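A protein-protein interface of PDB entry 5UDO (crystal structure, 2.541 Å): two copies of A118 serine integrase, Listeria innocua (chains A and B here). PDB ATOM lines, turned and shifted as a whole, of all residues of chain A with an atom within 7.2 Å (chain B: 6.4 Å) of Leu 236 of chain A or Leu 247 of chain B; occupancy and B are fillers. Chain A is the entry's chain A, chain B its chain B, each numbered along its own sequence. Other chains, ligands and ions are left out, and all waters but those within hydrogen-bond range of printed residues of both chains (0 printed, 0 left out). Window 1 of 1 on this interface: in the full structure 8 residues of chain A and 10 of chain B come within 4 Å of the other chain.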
ATOM      1  N   LYS A 231      -2.571  28.272 -23.395  1.00  0.00           N
ATOM      2  CA  LYS A 231      -3.209  29.533 -23.026  1.00  0.00           C
ATOM      3  C   LYS A 231      -4.218  29.352 -21.895  1.00  0.00           C
ATOM      4  O   LYS A 231      -4.221  30.116 -20.931  1.00  0.00           O
ATOM      5  CB  LYS A 231      -3.898  30.159 -24.240  1.00  0.00           C
ATOM      6  CG  LYS A 231      -4.610  31.473 -23.950  1.00  0.00           C
ATOM      7  CD  LYS A 231      -5.231  32.053 -25.213  1.00  0.00           C
ATOM      8  CE  LYS A 231      -5.939  33.370 -24.935  1.00  0.00           C
ATOM      9  NZ  LYS A 231      -6.525  33.967 -26.169  1.00  0.00           N
ATOM     10  N   ARG A 232      -5.072  28.339 -22.018  1.00  0.00           N
ATOM     11  CA  ARG A 232      -6.101  28.078 -21.014  1.00  0.00           C
ATOM     12  C   ARG A 232      -5.492  27.667 -19.678  1.00  0.00           C
ATOM     13  O   ARG A 232      -6.027  27.992 -18.618  1.00  0.00           O
ATOM     14  CB  ARG A 232      -7.066  26.993 -21.493  1.00  0.00           C
ATOM     15  CG  ARG A 232      -7.757  27.297 -22.812  1.00  0.00           C
ATOM     16  CD  ARG A 232      -9.070  26.537 -22.929  1.00  0.00           C
ATOM     17  NE  ARG A 232     -10.223  27.400 -22.681  1.00  0.00           N
ATOM     18  CZ  ARG A 232     -11.378  26.987 -22.167  1.00  0.00           C
ATOM     19  NH1 ARG A 232     -11.544  25.717 -21.826  1.00  0.00           N
ATOM     20  NH2 ARG A 232     -12.367  27.849 -21.983  1.00  0.00           N
ATOM     21  N   LEU A 233      -4.376  26.946 -19.737  1.00  0.00           N
ATOM     22  CA  LEU A 233      -3.703  26.483 -18.531  1.00  0.00           C
ATOM     23  C   LEU A 233      -3.136  27.651 -17.728  1.00  0.00           C
ATOM     24  O   LEU A 233      -3.104  27.610 -16.498  1.00  0.00           O
ATOM     25  CB  LEU A 233      -2.588  25.495 -18.882  1.00  0.00           C
ATOM     26  CG  LEU A 233      -1.863  24.858 -17.694  1.00  0.00           C
ATOM     27  CD1 LEU A 233      -2.851  24.124 -16.801  1.00  0.00           C
ATOM     28  CD2 LEU A 233      -0.760  23.919 -18.160  1.00  0.00           C
ATOM     29  N   PHE A 234      -2.700  28.694 -18.427  1.00  0.00           N
ATOM     30  CA  PHE A 234      -2.083  29.843 -17.775  1.00  0.00           C
ATOM     31  C   PHE A 234      -3.086  30.634 -16.933  1.00  0.00           C
ATOM     32  O   PHE A 234      -2.711  31.272 -15.950  1.00  0.00           O
ATOM     33  CB  PHE A 234      -1.435  30.760 -18.813  1.00  0.00           C
ATOM     34  CG  PHE A 234      -0.515  31.792 -18.221  1.00  0.00           C
ATOM     35  CD1 PHE A 234       0.807  31.486 -17.947  1.00  0.00           C
ATOM     36  CD2 PHE A 234      -0.972  33.069 -17.940  1.00  0.00           C
ATOM     37  CE1 PHE A 234       1.653  32.430 -17.402  1.00  0.00           C
ATOM     38  CE2 PHE A 234      -0.130  34.017 -17.395  1.00  0.00           C
ATOM     39  CZ  PHE A 234       1.183  33.698 -17.126  1.00  0.00           C
ATOM     40  N   ASP A 235      -4.357  30.586 -17.322  1.00  0.00           N
ATOM     41  CA  ASP A 235      -5.408  31.310 -16.613  1.00  0.00           C
ATOM     42  C   ASP A 235      -5.611  30.756 -15.205  1.00  0.00           C
ATOM     43  O   ASP A 235      -5.943  31.494 -14.276  1.00  0.00           O
ATOM     44  CB  ASP A 235      -6.720  31.251 -17.400  1.00  0.00           C
ATOM     45  CG  ASP A 235      -6.597  31.852 -18.789  1.00  0.00           C
ATOM     46  OD1 ASP A 235      -5.459  31.982 -19.284  1.00  0.00           O
ATOM     47  OD2 ASP A 235      -7.641  32.191 -19.388  1.00  0.00           O
ATOM     48  N   LEU A 236      -5.392  29.453 -15.051  1.00  0.00           N
ATOM     49  CA  LEU A 236      -5.588  28.772 -13.774  1.00  0.00           C
ATOM     50  C   LEU A 236      -4.584  29.238 -12.720  1.00  0.00           C
ATOM     51  O   LEU A 236      -4.794  29.059 -11.518  1.00  0.00           O
ATOM     52  CB  LEU A 236      -5.477  27.258 -13.964  1.00  0.00           C
ATOM     53  CG  LEU A 236      -6.341  26.664 -15.078  1.00  0.00           C
ATOM     54  CD1 LEU A 236      -6.172  25.156 -15.156  1.00  0.00           C
ATOM     55  CD2 LEU A 236      -7.802  27.031 -14.874  1.00  0.00           C
ATOM     56  N   TYR A 237      -3.489  29.832 -13.183  1.00  0.00           N
ATOM     57  CA  TYR A 237      -2.423  30.300 -12.301  1.00  0.00           C
ATOM     58  C   TYR A 237      -2.820  31.524 -11.481  1.00  0.00           C
ATOM     59  O   TYR A 237      -2.230  31.797 -10.436  1.00  0.00           O
ATOM     60  CB  TYR A 237      -1.161  30.616 -13.112  1.00  0.00           C
ATOM     61  CG  TYR A 237      -0.412  29.394 -13.595  1.00  0.00           C
ATOM     62  CD1 TYR A 237      -0.769  28.757 -14.771  1.00  0.00           C
ATOM     63  CD2 TYR A 237       0.659  28.884 -12.874  1.00  0.00           C
ATOM     64  CE1 TYR A 237      -0.084  27.641 -15.218  1.00  0.00           C
ATOM     65  CE2 TYR A 237       1.350  27.772 -13.310  1.00  0.00           C
ATOM     66  CZ  TYR A 237       0.975  27.156 -14.482  1.00  0.00           C
ATOM     67  OH  TYR A 237       1.661  26.049 -14.916  1.00  0.00           O
ATOM     68  N   ILE A 238      -3.826  32.254 -11.949  1.00  0.00           N
ATOM     69  CA  ILE A 238      -4.227  33.491 -11.288  1.00  0.00           C
ATOM     70  C   ILE A 238      -5.079  33.210 -10.048  1.00  0.00           C
ATOM     71  O   ILE A 238      -4.975  33.918  -9.045  1.00  0.00           O
ATOM     72  CB  ILE A 238      -4.999  34.418 -12.248  1.00  0.00           C
ATOM     73  CG1 ILE A 238      -4.282  34.509 -13.598  1.00  0.00           C
ATOM     74  CG2 ILE A 238      -5.172  35.796 -11.631  1.00  0.00           C
ATOM     75  CD1 ILE A 238      -2.871  35.052 -13.510  1.00  0.00           C
ATOM     76  N   ASN A 239      -5.917  32.179 -10.116  1.00  0.00           N
ATOM     77  CA  ASN A 239      -6.726  31.787  -8.962  1.00  0.00           C
ATOM     78  C   ASN A 239      -5.884  31.176  -7.846  1.00  0.00           C
ATOM     79  O   ASN A 239      -4.869  30.529  -8.105  1.00  0.00           O
ATOM     80  CB  ASN A 239      -7.818  30.798  -9.377  1.00  0.00           C
ATOM     81  CG  ASN A 239      -9.082  31.489  -9.849  1.00  0.00           C
ATOM     82  OD1 ASN A 239      -9.363  32.623  -9.462  1.00  0.00           O
ATOM     83  ND2 ASN A 239      -9.854  30.807 -10.689  1.00  0.00           N
ATOM     84  N   GLY A 240      -6.317  31.378  -6.605  1.00  0.00           N
ATOM     85  CA  GLY A 240      -5.642  30.805  -5.454  1.00  0.00           C
ATOM     86  C   GLY A 240      -5.876  29.310  -5.358  1.00  0.00           C
ATOM     87  O   GLY A 240      -5.154  28.597  -4.660  1.00  0.00           O
ATOM     88  N   SER A 241      -6.893  28.837  -6.070  1.00  0.00           N
ATOM     89  CA  SER A 241      -7.223  27.419  -6.102  1.00  0.00           C
ATOM     90  C   SER A 241      -6.175  26.610  -6.864  1.00  0.00           C
ATOM     91  O   SER A 241      -5.140  27.144  -7.272  1.00  0.00           O
ATOM     92  CB  SER A 241      -8.601  27.209  -6.731  1.00  0.00           C
ATOM     93  OG  SER A 241      -8.929  25.831  -6.789  1.00  0.00           O
ATOM     94  N   TYR A 242      -6.458  25.321  -7.042  1.00  0.00           N
ATOM     95  CA  TYR A 242      -5.575  24.389  -7.743  1.00  0.00           C
ATOM     96  C   TYR A 242      -4.211  24.259  -7.068  1.00  0.00           C
ATOM     97  O   TYR A 242      -3.947  24.878  -6.037  1.00  0.00           O
ATOM     98  CB  TYR A 242      -5.387  24.811  -9.203  1.00  0.00           C
ATOM     99  CG  TYR A 242      -6.665  25.217  -9.899  1.00  0.00           C
ATOM    100  CD1 TYR A 242      -7.575  24.265 -10.333  1.00  0.00           C
ATOM    101  CD2 TYR A 242      -6.955  26.555 -10.129  1.00  0.00           C
ATOM    102  CE1 TYR A 242      -8.744  24.635 -10.971  1.00  0.00           C
ATOM    103  CE2 TYR A 242      -8.119  26.935 -10.765  1.00  0.00           C
ATOM    104  CZ  TYR A 242      -9.010  25.971 -11.185  1.00  0.00           C
ATOM    105  OH  TYR A 242     -10.169  26.350 -11.819  1.00  0.00           O
ATOM    106  N   GLU A 243      -3.350  23.438  -7.658  1.00  0.00           N
ATOM    107  CA  GLU A 243      -1.994  23.263  -7.160  1.00  0.00           C
ATOM    108  C   GLU A 243      -0.997  23.493  -8.288  1.00  0.00           C
ATOM    109  O   GLU A 243      -1.168  22.977  -9.394  1.00  0.00           O
ATOM    110  CB  GLU A 243      -1.810  21.870  -6.553  1.00  0.00           C
ATOM    111  CG  GLU A 243      -0.419  21.606  -5.985  1.00  0.00           C
ATOM    112  CD  GLU A 243      -0.090  22.469  -4.778  1.00  0.00           C
ATOM    113  OE1 GLU A 243      -1.025  22.964  -4.114  1.00  0.00           O
ATOM    114  OE2 GLU A 243       1.113  22.650  -4.490  1.00  0.00           O
ATOM    115  N   LEU A 247      -0.247  22.030 -12.382  1.00  0.00           N
ATOM    116  CA  LEU A 247      -0.197  22.905 -13.547  1.00  0.00           C
ATOM    117  C   LEU A 247       1.163  22.845 -14.237  1.00  0.00           C
ATOM    118  O   LEU A 247       1.241  22.755 -15.462  1.00  0.00           O
ATOM    119  CB  LEU A 247      -0.522  24.342 -13.141  1.00  0.00           C
ATOM    120  CG  LEU A 247      -1.834  24.544 -12.377  1.00  0.00           C
ATOM    121  CD1 LEU A 247      -2.084  26.021 -12.120  1.00  0.00           C
ATOM    122  CD2 LEU A 247      -3.002  23.920 -13.126  1.00  0.00           C
ATOM    123  N   MET A 250       1.651  19.538 -16.103  1.00  0.00           N
ATOM    124  CA  MET A 250       0.923  19.562 -17.365  1.00  0.00           C
ATOM    125  C   MET A 250       1.590  20.518 -18.346  1.00  0.00           C
ATOM    126  O   MET A 250       1.720  20.210 -19.533  1.00  0.00           O
ATOM    127  CB  MET A 250      -0.533  19.960 -17.135  1.00  0.00           C
ATOM    128  CG  MET A 250      -1.328  18.922 -16.350  1.00  0.00           C
ATOM    129  SD  MET A 250      -3.003  19.454 -15.962  1.00  0.00           S
ATOM    130  CE  MET A 250      -3.618  18.011 -15.102  1.00  0.00           C
ATOM    131  N   LEU B 233     -10.316  16.217 -16.266  1.00  0.00           N
ATOM    132  CA  LEU B 233     -11.080  17.458 -16.149  1.00  0.00           C
ATOM    133  C   LEU B 233     -10.251  18.661 -16.585  1.00  0.00           C
ATOM    134  O   LEU B 233     -10.752  19.548 -17.277  1.00  0.00           O
ATOM    135  CB  LEU B 233     -11.578  17.654 -14.716  1.00  0.00           C
ATOM    136  CG  LEU B 233     -12.445  18.892 -14.472  1.00  0.00           C
ATOM    137  CD1 LEU B 233     -13.590  18.949 -15.473  1.00  0.00           C
ATOM    138  CD2 LEU B 233     -12.981  18.912 -13.048  1.00  0.00           C
ATOM    139  N   PHE B 234      -8.985  18.687 -16.178  1.00  0.00           N
ATOM    140  CA  PHE B 234      -8.062  19.712 -16.644  1.00  0.00           C
ATOM    141  C   PHE B 234      -7.908  19.622 -18.157  1.00  0.00           C
ATOM    142  O   PHE B 234      -7.954  20.634 -18.854  1.00  0.00           O
ATOM    143  CB  PHE B 234      -6.695  19.571 -15.971  1.00  0.00           C
ATOM    144  CG  PHE B 234      -6.605  20.225 -14.620  1.00  0.00           C
ATOM    145  CD1 PHE B 234      -6.741  21.596 -14.488  1.00  0.00           C
ATOM    146  CD2 PHE B 234      -6.352  19.471 -13.486  1.00  0.00           C
ATOM    147  CE1 PHE B 234      -6.647  22.201 -13.247  1.00  0.00           C
ATOM    148  CE2 PHE B 234      -6.254  20.069 -12.243  1.00  0.00           C
ATOM    149  CZ  PHE B 234      -6.401  21.435 -12.123  1.00  0.00           C
ATOM    150  N   TYR B 237     -11.041  20.915 -19.989  1.00  0.00           N
ATOM    151  CA  TYR B 237     -11.005  22.372 -19.956  1.00  0.00           C
ATOM    152  C   TYR B 237      -9.984  22.917 -20.945  1.00  0.00           C
ATOM    153  O   TYR B 237     -10.292  23.799 -21.749  1.00  0.00           O
ATOM    154  CB  TYR B 237     -10.681  22.865 -18.545  1.00  0.00           C
ATOM    155  CG  TYR B 237     -10.195  24.294 -18.499  1.00  0.00           C
ATOM    156  CD1 TYR B 237     -11.087  25.352 -18.594  1.00  0.00           C
ATOM    157  CD2 TYR B 237      -8.844  24.585 -18.363  1.00  0.00           C
ATOM    158  CE1 TYR B 237     -10.649  26.658 -18.559  1.00  0.00           C
ATOM    159  CE2 TYR B 237      -8.396  25.888 -18.326  1.00  0.00           C
ATOM    160  CZ  TYR B 237      -9.302  26.921 -18.423  1.00  0.00           C
ATOM    161  OH  TYR B 237      -8.859  28.222 -18.386  1.00  0.00           O
ATOM    162  N   ILE B 238      -8.769  22.379 -20.867  1.00  0.00           N
ATOM    163  CA  ILE B 238      -7.669  22.752 -21.750  1.00  0.00           C
ATOM    164  C   ILE B 238      -8.066  22.603 -23.218  1.00  0.00           C
ATOM    165  O   ILE B 238      -7.716  23.437 -24.056  1.00  0.00           O
ATOM    166  CB  ILE B 238      -6.411  21.900 -21.453  1.00  0.00           C
ATOM    167  CG1 ILE B 238      -5.725  22.388 -20.173  1.00  0.00           C
ATOM    168  CG2 ILE B 238      -5.439  21.933 -22.613  1.00  0.00           C
ATOM    169  CD1 ILE B 238      -4.483  21.613 -19.799  1.00  0.00           C
ATOM    170  N   TYR B 242     -14.785  22.982 -21.551  1.00  0.00           N
ATOM    171  CA  TYR B 242     -15.397  23.660 -20.413  1.00  0.00           C
ATOM    172  C   TYR B 242     -14.740  25.006 -20.133  1.00  0.00           C
ATOM    173  O   TYR B 242     -13.609  25.252 -20.550  1.00  0.00           O
ATOM    174  CB  TYR B 242     -15.323  22.781 -19.163  1.00  0.00           C
ATOM    175  CG  TYR B 242     -16.467  21.805 -19.035  1.00  0.00           C
ATOM    176  CD1 TYR B 242     -17.728  22.123 -19.519  1.00  0.00           C
ATOM    177  CD2 TYR B 242     -16.289  20.565 -18.433  1.00  0.00           C
ATOM    178  CE1 TYR B 242     -18.780  21.237 -19.407  1.00  0.00           C
ATOM    179  CE2 TYR B 242     -17.337  19.672 -18.318  1.00  0.00           C
ATOM    180  CZ  TYR B 242     -18.581  20.014 -18.807  1.00  0.00           C
ATOM    181  OH  TYR B 242     -19.629  19.132 -18.697  1.00  0.00           O
ATOM    182  N   GLU B 243     -15.455  25.873 -19.422  1.00  0.00           N
ATOM    183  CA  GLU B 243     -14.923  27.177 -19.043  1.00  0.00           C
ATOM    184  C   GLU B 243     -14.395  27.140 -17.613  1.00  0.00           C
ATOM    185  O   GLU B 243     -14.595  26.159 -16.899  1.00  0.00           O
ATOM    186  CB  GLU B 243     -15.994  28.262 -19.180  1.00  0.00           C
ATOM    187  CG  GLU B 243     -16.721  28.274 -20.524  1.00  0.00           C
ATOM    188  CD  GLU B 243     -15.861  28.780 -21.670  1.00  0.00           C
ATOM    189  OE1 GLU B 243     -16.345  28.769 -22.822  1.00  0.00           O
ATOM    190  OE2 GLU B 243     -14.707  29.193 -21.427  1.00  0.00           O
ATOM    191  N   VAL B 244     -13.723  28.213 -17.201  1.00  0.00           N
ATOM    192  CA  VAL B 244     -13.143  28.298 -15.863  1.00  0.00           C
ATOM    193  C   VAL B 244     -14.218  28.267 -14.782  1.00  0.00           C
ATOM    194  O   VAL B 244     -14.091  27.543 -13.795  1.00  0.00           O
ATOM    195  CB  VAL B 244     -12.303  29.578 -15.690  1.00  0.00           C
ATOM    196  CG1 VAL B 244     -11.661  29.607 -14.310  1.00  0.00           C
ATOM    197  CG2 VAL B 244     -11.244  29.666 -16.771  1.00  0.00           C
ATOM    198  N   SER B 245     -15.270  29.057 -14.979  1.00  0.00           N
ATOM    199  CA  SER B 245     -16.358  29.174 -14.010  1.00  0.00           C
ATOM    200  C   SER B 245     -16.955  27.816 -13.650  1.00  0.00           C
ATOM    201  O   SER B 245     -17.120  27.495 -12.473  1.00  0.00           O
ATOM    202  CB  SER B 245     -17.453  30.093 -14.552  1.00  0.00           C
ATOM    203  OG  SER B 245     -18.010  29.572 -15.746  1.00  0.00           O
ATOM    204  N   GLU B 246     -17.274  27.025 -14.669  1.00  0.00           N
ATOM    205  CA  GLU B 246     -17.811  25.687 -14.454  1.00  0.00           C
ATOM    206  C   GLU B 246     -16.722  24.733 -13.972  1.00  0.00           C
ATOM    207  O   GLU B 246     -16.999  23.789 -13.230  1.00  0.00           O
ATOM    208  CB  GLU B 246     -18.454  25.155 -15.735  1.00  0.00           C
ATOM    209  CG  GLU B 246     -19.731  25.881 -16.136  1.00  0.00           C
ATOM    210  CD  GLU B 246     -20.312  25.366 -17.439  1.00  0.00           C
ATOM    211  OE1 GLU B 246     -19.524  25.025 -18.348  1.00  0.00           O
ATOM    212  OE2 GLU B 246     -21.553  25.295 -17.554  1.00  0.00           O
ATOM    213  N   LEU B 247     -15.486  24.986 -14.391  1.00  0.00           N
ATOM    214  CA  LEU B 247     -14.349  24.171 -13.977  1.00  0.00           C
ATOM    215  C   LEU B 247     -14.120  24.256 -12.472  1.00  0.00           C
ATOM    216  O   LEU B 247     -13.901  23.242 -11.811  1.00  0.00           O
ATOM    217  CB  LEU B 247     -13.080  24.601 -14.715  1.00  0.00           C
ATOM    218  CG  LEU B 247     -11.785  23.877 -14.344  1.00  0.00           C
ATOM    219  CD1 LEU B 247     -11.800  22.454 -14.875  1.00  0.00           C
ATOM    220  CD2 LEU B 247     -10.569  24.635 -14.854  1.00  0.00           C
ATOM    221  N   ASP B 248     -14.173  25.476 -11.944  1.00  0.00           N
ATOM    222  CA  ASP B 248     -13.914  25.730 -10.528  1.00  0.00           C
ATOM    223  C   ASP B 248     -14.861  24.953  -9.623  1.00  0.00           C
ATOM    224  O   ASP B 248     -14.422  24.222  -8.735  1.00  0.00           O
ATOM    225  CB  ASP B 248     -14.029  27.225 -10.226  1.00  0.00           C
ATOM    226  CG  ASP B 248     -13.053  28.059 -11.028  1.00  0.00           C
ATOM    227  OD1 ASP B 248     -12.056  27.496 -11.524  1.00  0.00           O
ATOM    228  OD2 ASP B 248     -13.281  29.281 -11.161  1.00  0.00           O
ATOM    229  N   SER B 249     -16.159  25.122  -9.854  1.00  0.00           N
ATOM    230  CA  SER B 249     -17.178  24.460  -9.052  1.00  0.00           C
ATOM    231  C   SER B 249     -17.026  22.942  -9.115  1.00  0.00           C
ATOM    232  O   SER B 249     -17.172  22.256  -8.105  1.00  0.00           O
ATOM    233  CB  SER B 249     -18.576  24.871  -9.517  1.00  0.00           C
ATOM    234  OG  SER B 249     -18.817  24.458 -10.851  1.00  0.00           O
ATOM    235  N   MET B 250     -16.721  22.427 -10.301  1.00  0.00           N
ATOM    236  CA  MET B 250     -16.525  20.992 -10.488  1.00  0.00           C
ATOM    237  C   MET B 250     -15.256  20.505  -9.800  1.00  0.00           C
ATOM    238  O   MET B 250     -15.291  19.546  -9.027  1.00  0.00           O
ATOM    239  CB  MET B 250     -16.474  20.647 -11.974  1.00  0.00           C
ATOM    240  CG  MET B 250     -17.810  20.749 -12.679  1.00  0.00           C
ATOM    241  SD  MET B 250     -17.689  20.402 -14.442  1.00  0.00           S
ATOM    242  CE  MET B 250     -19.410  20.515 -14.920  1.00  0.00           C
ATOM    243  N   MET B 251     -14.141  21.170 -10.091  1.00  0.00           N
ATOM    244  CA  MET B 251     -12.849  20.820  -9.509  1.00  0.00           C
ATOM    245  C   MET B 251     -12.902  20.857  -7.985  1.00  0.00           C
ATOM    246  O   MET B 251     -12.359  19.976  -7.316  1.00  0.00           O
ATOM    247  CB  MET B 251     -11.760  21.766 -10.012  1.00  0.00           C
ATOM    248  CG  MET B 251     -10.366  21.407  -9.535  1.00  0.00           C
ATOM    249  SD  MET B 251      -9.744  19.916 -10.328  1.00  0.00           S
ATOM    250  CE  MET B 251      -9.816  20.412 -12.048  1.00  0.00           C
ATOM    251  N   ASN B 252     -13.562  21.877  -7.442  1.00  0.00           N
ATOM    252  CA  ASN B 252     -13.729  21.999  -6.000  1.00  0.00           C
ATOM    253  C   ASN B 252     -14.611  20.889  -5.440  1.00  0.00           C
ATOM    254  O   ASN B 252     -14.327  20.345  -4.376  1.00  0.00           O
ATOM    255  CB  ASN B 252     -14.320  23.363  -5.637  1.00  0.00           C
ATOM    256  CG  ASN B 252     -13.298  24.481  -5.712  1.00  0.00           C
ATOM    257  OD1 ASN B 252     -12.778  24.932  -4.691  1.00  0.00           O
ATOM    258  ND2 ASN B 252     -13.009  24.937  -6.924  1.00  0.00           N
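The backbone carbonyl oxygen (O) of Asp 248 of chain B sits at hydrogen-bond distance from the side-chain amide nitrogen (ND2) of Asn 252 of chain B (2.4 Å).
Among the printed residues, pairs that only touch across the chains: Arg 232 of chain A with Ile 238 of chain B (3.6 Å), Asp 235 of chain A with Tyr 237 of chain B (3.8 Å), Leu 236 of chain A with Phe 234 of chain B (3.5 Å), Leu 236 of chain A with Tyr 237 of chain B (3.7 Å), Leu 236 of chain A with Leu 247 of chain B (3.7 Å), Asn 239 of chain A with Asp 248 of chain B (3.8 Å), Tyr 242 of chain A with Phe 234 of chain B (3.5 Å), Tyr 242 of chain A with Leu 247 of chain B (3.5 Å), Tyr 242 of chain A with Met 251 of chain B (3.9 Å) and Met 250 of chain A with Phe 234 of chain B (3.5 Å).
Printed residues of chain B within 4 Å of Tyr 242 of chain A: Phe 234, Leu 247, Asp 248 and Met 251.
Of the printed residues of chain A, Ile 238 of chain B touches Arg 232.
Leu 247 of chain B touches just these residues of chain A: Leu 236 (3.7 Å) and Tyr 242 (3.5 Å).
Tyr 242 of chain A touches Phe 234 of chain B, but with the chains exchanged Phe 234 of chain A does not touch Tyr 242 of chain B (11.6 Å).
Tyr 242 of chain A touches Leu 247 of chain B, but with the chains exchanged Leu 247 of chain A does not touch Tyr 242 of chain B (13.0 Å).
Met 250 of chain A touches Phe 234 of chain B, but with the chains exchanged Phe 234 of chain A does not touch Met 250 of chain B (17.2 Å).
8 positions are printed for both chains.
OH of Tyr 237 of chain B is in hydrogen-bond range of O of Arg 232 of chain A, at 2.9 Å.
The backbone carbonyl oxygen (O) of Tyr 242 of chain B is in hydrogen-bond range of the guanidinium group (NH1) of Arg 232 of chain A (2.5 Å).
The guanidinium group of Arg 232 of chain A is in salt-bridge range of the side-chain carboxylate of Glu 243 of chain B (2.8 Å).
OD1 of Asp 248 of chain B lies close to OH of Tyr 242 of chain A.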
